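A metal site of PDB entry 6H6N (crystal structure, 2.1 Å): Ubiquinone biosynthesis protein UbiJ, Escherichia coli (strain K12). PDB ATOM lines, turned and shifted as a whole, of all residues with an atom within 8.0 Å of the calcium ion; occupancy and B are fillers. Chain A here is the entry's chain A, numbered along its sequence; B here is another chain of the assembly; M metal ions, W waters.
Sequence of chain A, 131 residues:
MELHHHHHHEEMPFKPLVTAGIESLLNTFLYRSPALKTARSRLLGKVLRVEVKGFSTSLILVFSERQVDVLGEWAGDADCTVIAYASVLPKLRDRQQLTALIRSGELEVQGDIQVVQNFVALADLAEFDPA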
ATOM      1  N   THR A  28      -9.104 -30.946   8.858  1.00  0.00           N
ATOM      2  CA  THR A  28      -8.521 -31.515   7.630  1.00  0.00           C
ATOM      3  C   THR A  28      -7.100 -30.940   7.437  1.00  0.00           C
ATOM      4  O   THR A  28      -6.181 -31.679   7.093  1.00  0.00           O
ATOM      5  CB  THR A  28      -9.407 -31.245   6.408  1.00  0.00           C
ATOM      6  OG1 THR A  28     -10.750 -31.610   6.709  1.00  0.00           O
ATOM      7  CG2 THR A  28      -8.915 -31.987   5.148  1.00  0.00           C
ATOM      8  N   PHE A  29      -6.939 -29.639   7.656  1.00  0.00           N
ATOM      9  CA  PHE A  29      -5.669 -28.948   7.455  1.00  0.00           C
ATOM     10  C   PHE A  29      -4.596 -29.274   8.493  1.00  0.00           C
ATOM     11  O   PHE A  29      -3.422 -29.458   8.115  1.00  0.00           O
ATOM     12  CB  PHE A  29      -5.904 -27.432   7.381  1.00  0.00           C
ATOM     13  CG  PHE A  29      -4.691 -26.591   7.060  1.00  0.00           C
ATOM     14  CD1 PHE A  29      -3.965 -26.808   5.891  1.00  0.00           C
ATOM     15  CD2 PHE A  29      -4.291 -25.542   7.894  1.00  0.00           C
ATOM     16  CE1 PHE A  29      -2.835 -26.028   5.589  1.00  0.00           C
ATOM     17  CE2 PHE A  29      -3.179 -24.755   7.587  1.00  0.00           C
ATOM     18  CZ  PHE A  29      -2.452 -25.014   6.437  1.00  0.00           C
ATOM     19  N   LEU A  30      -4.973 -29.327   9.792  1.00  0.00           N
ATOM     20  CA  LEU A  30      -4.011 -29.514  10.876  1.00  0.00           C
ATOM     21  C   LEU A  30      -3.954 -30.887  11.503  1.00  0.00           C
ATOM     22  O   LEU A  30      -2.888 -31.269  11.982  1.00  0.00           O
ATOM     23  CB  LEU A  30      -4.279 -28.480  11.994  1.00  0.00           C
ATOM     24  CG  LEU A  30      -4.357 -27.002  11.530  1.00  0.00           C
ATOM     25  CD1 LEU A  30      -4.886 -26.145  12.628  1.00  0.00           C
ATOM     26  CD2 LEU A  30      -2.967 -26.475  11.020  1.00  0.00           C
ATOM     27  N   ARG A  32      -5.192 -34.067  10.022  1.00  0.00           N
ATOM     28  CA  ARG A  32      -5.179 -35.256   9.170  1.00  0.00           C
ATOM     29  C   ARG A  32      -3.795 -35.931   9.140  1.00  0.00           C
ATOM     30  O   ARG A  32      -3.711 -37.157   9.205  1.00  0.00           O
ATOM     31  CB  ARG A  32      -5.683 -34.940   7.756  1.00  0.00           C
ATOM     32  CG  ARG A  32      -6.073 -36.176   6.949  1.00  0.00           C
ATOM     33  CD  ARG A  32      -6.637 -35.818   5.578  1.00  0.00           C
ATOM     34  NE  ARG A  32      -7.073 -37.014   4.849  1.00  0.00           N
ATOM     35  CZ  ARG A  32      -8.296 -37.523   4.918  1.00  0.00           C
ATOM     36  NH1 ARG A  32      -8.599 -38.626   4.235  1.00  0.00           N
ATOM     37  NH2 ARG A  32      -9.236 -36.952   5.673  1.00  0.00           N
ATOM     38  N   SER A  33      -2.733 -35.147   9.083  1.00  0.00           N
ATOM     39  CA  SER A  33      -1.397 -35.688   9.009  1.00  0.00           C
ATOM     40  C   SER A  33      -0.758 -36.055  10.373  1.00  0.00           C
ATOM     41  O   SER A  33      -0.485 -35.174  11.188  1.00  0.00           O
ATOM     42  CB  SER A  33      -0.475 -34.750   8.228  1.00  0.00           C
ATOM     43  OG  SER A  33       0.816 -35.314   8.170  1.00  0.00           O
ATOM     44  N   LEU A  36       2.496 -34.107  11.820  1.00  0.00           N
ATOM     45  CA  LEU A  36       2.354 -32.880  12.632  1.00  0.00           C
ATOM     46  C   LEU A  36       2.131 -33.126  14.119  1.00  0.00           C
ATOM     47  O   LEU A  36       1.996 -32.162  14.849  1.00  0.00           O
ATOM     48  CB  LEU A  36       1.219 -31.977  12.082  1.00  0.00           C
ATOM     49  CG  LEU A  36       1.375 -31.534  10.640  1.00  0.00           C
ATOM     50  CD1 LEU A  36       0.151 -30.746  10.189  1.00  0.00           C
ATOM     51  CD2 LEU A  36       2.687 -30.729  10.445  1.00  0.00           C
ATOM     52  N   LEU A 122       2.343 -24.313  13.935  1.00  0.00           N
ATOM     53  CA  LEU A 122       1.641 -25.518  13.473  1.00  0.00           C
ATOM     54  C   LEU A 122       1.122 -25.339  12.041  1.00  0.00           C
ATOM     55  O   LEU A 122       1.385 -26.185  11.196  1.00  0.00           O
ATOM     56  CB  LEU A 122       0.464 -25.892  14.433  1.00  0.00           C
ATOM     57  CG  LEU A 122      -0.515 -27.015  13.970  1.00  0.00           C
ATOM     58  CD1 LEU A 122       0.183 -28.326  13.721  1.00  0.00           C
ATOM     59  CD2 LEU A 122      -1.631 -27.234  14.972  1.00  0.00           C
ATOM     60  N   ALA A 123       0.396 -24.222  11.776  1.00  0.00           N
ATOM     61  CA  ALA A 123      -0.180 -23.885  10.469  1.00  0.00           C
ATOM     62  C   ALA A 123       0.908 -23.768   9.420  1.00  0.00           C
ATOM     63  O   ALA A 123       0.702 -24.216   8.286  1.00  0.00           O
ATOM     64  CB  ALA A 123      -0.988 -22.592  10.548  1.00  0.00           C
ATOM     65  N   ASP A 124       2.081 -23.214   9.809  1.00  0.00           N
ATOM     66  CA  ASP A 124       3.241 -23.063   8.930  1.00  0.00           C
ATOM     67  C   ASP A 124       3.828 -24.452   8.564  1.00  0.00           C
ATOM     68  O   ASP A 124       4.126 -24.719   7.407  1.00  0.00           O
ATOM     69  CB  ASP A 124       4.305 -22.149   9.571  1.00  0.00           C
ATOM     70  CG  ASP A 124       5.416 -21.701   8.638  1.00  0.00           C
ATOM     71  OD1 ASP A 124       5.286 -21.899   7.406  1.00  0.00           O
ATOM     72  OD2 ASP A 124       6.434 -21.134   9.142  1.00  0.00           O
ATOM     73  N   LEU A 125       3.931 -25.343   9.539  1.00  0.00           N
ATOM     74  CA  LEU A 125       4.395 -26.700   9.280  1.00  0.00           C
ATOM     75  C   LEU A 125       3.356 -27.542   8.516  1.00  0.00           C
ATOM     76  O   LEU A 125       3.742 -28.485   7.823  1.00  0.00           O
ATOM     77  CB  LEU A 125       4.778 -27.393  10.593  1.00  0.00           C
ATOM     78  CG  LEU A 125       6.059 -26.885  11.235  1.00  0.00           C
ATOM     79  CD1 LEU A 125       6.135 -27.326  12.675  1.00  0.00           C
ATOM     80  CD2 LEU A 125       7.277 -27.384  10.492  1.00  0.00           C
ATOM     81  N   ALA A 126       2.049 -27.183   8.630  1.00  0.00           N
ATOM     82  CA  ALA A 126       0.950 -27.882   7.932  1.00  0.00           C
ATOM     83  C   ALA A 126       1.006 -27.624   6.426  1.00  0.00           C
ATOM     84  O   ALA A 126       0.537 -28.453   5.641  1.00  0.00           O
ATOM     85  CB  ALA A 126      -0.394 -27.450   8.501  1.00  0.00           C
ATOM     86  N   GLU A 127       1.583 -26.471   6.051  1.00  0.00           N
ATOM     87  CA  GLU A 127       1.812 -26.029   4.672  1.00  0.00           C
ATOM     88  C   GLU A 127       3.047 -26.741   4.108  1.00  0.00           C
ATOM     89  O   GLU A 127       3.063 -27.069   2.926  1.00  0.00           O
ATOM     90  CB  GLU A 127       2.018 -24.505   4.649  1.00  0.00           C
ATOM     91  CG  GLU A 127       1.908 -23.891   3.263  1.00  0.00           C
ATOM     92  CD  GLU A 127       2.585 -22.540   3.063  1.00  0.00           C
ATOM     93  OE1 GLU A 127       2.311 -21.609   3.859  1.00  0.00           O
ATOM     94  OE2 GLU A 127       3.340 -22.399   2.068  1.00  0.00           O
ATOM     95  N   PHE A 128       4.097 -26.962   4.956  1.00  0.00           N
ATOM     96  CA  PHE A 128       5.353 -27.616   4.580  1.00  0.00           C
ATOM     97  C   PHE A 128       5.113 -29.104   4.343  1.00  0.00           C
ATOM     98  O   PHE A 128       5.709 -29.712   3.456  1.00  0.00           O
ATOM     99  CB  PHE A 128       6.445 -27.411   5.662  1.00  0.00           C
ATOM    100  CG  PHE A 128       7.430 -28.565   5.792  1.00  0.00           C
ATOM    101  CD1 PHE A 128       8.470 -28.717   4.880  1.00  0.00           C
ATOM    102  CD2 PHE A 128       7.256 -29.548   6.769  1.00  0.00           C
ATOM    103  CE1 PHE A 128       9.324 -29.825   4.948  1.00  0.00           C
ATOM    104  CE2 PHE A 128       8.101 -30.653   6.834  1.00  0.00           C
ATOM    105  CZ  PHE A 128       9.138 -30.781   5.928  1.00  0.00           C
ATOM    106  N   ASP A 129       4.315 -29.688   5.220  1.00  0.00           N
ATOM    107  CA  ASP A 129       3.988 -31.105   5.182  1.00  0.00           C
ATOM    108  C   ASP A 129       3.041 -31.318   3.992  1.00  0.00           C
ATOM    109  O   ASP A 129       1.950 -30.765   4.022  1.00  0.00           O
ATOM    110  CB  ASP A 129       3.346 -31.492   6.502  1.00  0.00           C
ATOM    111  CG  ASP A 129       2.900 -32.915   6.537  1.00  0.00           C
ATOM    112  OD1 ASP A 129       3.497 -33.739   5.847  1.00  0.00           O
ATOM    113  OD2 ASP A 129       1.972 -33.214   7.266  1.00  0.00           O
ATOM    114  N   PRO A 130       3.463 -32.021   2.898  1.00  0.00           N
ATOM    115  CA  PRO A 130       2.594 -32.114   1.707  1.00  0.00           C
ATOM    116  C   PRO A 130       1.310 -32.923   1.876  1.00  0.00           C
ATOM    117  O   PRO A 130       0.401 -32.768   1.065  1.00  0.00           O
ATOM    118  CB  PRO A 130       3.509 -32.671   0.626  1.00  0.00           C
ATOM    119  CG  PRO A 130       4.576 -33.362   1.340  1.00  0.00           C
ATOM    120  CD  PRO A 130       4.753 -32.692   2.675  1.00  0.00           C
ATOM    121  N   ALA A 131       1.201 -33.724   2.963  1.00  0.00           N
ATOM    122  CA  ALA A 131       0.009 -34.508   3.287  1.00  0.00           C
ATOM    123  C   ALA A 131      -1.214 -33.583   3.502  1.00  0.00           C
ATOM    124  O   ALA A 131      -1.173 -32.668   4.333  1.00  0.00           O
ATOM    125  CB  ALA A 131       0.255 -35.350   4.523  1.00  0.00           C
ATOM    126  N   LEU B  17      -9.656 -26.674  -0.070  1.00  0.00           N
ATOM    127  CA  LEU B  17     -10.240 -26.877   1.254  1.00  0.00           C
ATOM    128  C   LEU B  17     -11.185 -25.725   1.679  1.00  0.00           C
ATOM    129  O   LEU B  17     -12.291 -25.959   2.158  1.00  0.00           O
ATOM    130  CB  LEU B  17      -9.090 -27.055   2.255  1.00  0.00           C
ATOM    131  CG  LEU B  17      -9.263 -28.112   3.339  1.00  0.00           C
ATOM    132  CD1 LEU B  17      -9.948 -29.378   2.798  1.00  0.00           C
ATOM    133  CD2 LEU B  17      -7.915 -28.427   3.986  1.00  0.00           C
HETATM  134 CA    CA M   1      -0.249 -30.368   4.621  1.00  0.00          CA
HETATM  135  O   HOH W   1      -2.301 -29.630   5.652  1.00  0.00           O
HETATM  136  O   HOH W   2      -0.220 -31.587   6.657  1.00  0.00           O
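The side-chain carboxylate of Asp 129 lies within hydrogen-bond range of the side-chain hydroxyl of Ser 33, at 2.6 Å.
The calcium ion is bound by O of Ala 126, 2.3 Å away. O of Asp 129 binds the calcium ion (2.3 Å). The calcium ion is bound by water W2 (2.4 Å). Water W1 binds the calcium ion (2.4 Å). The calcium ion is bound by the backbone carbonyl oxygen (O) of Ala 131 (2.5 Å).
Of the 17 residues printed, 3 come within 4 Å of the calcium ion.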
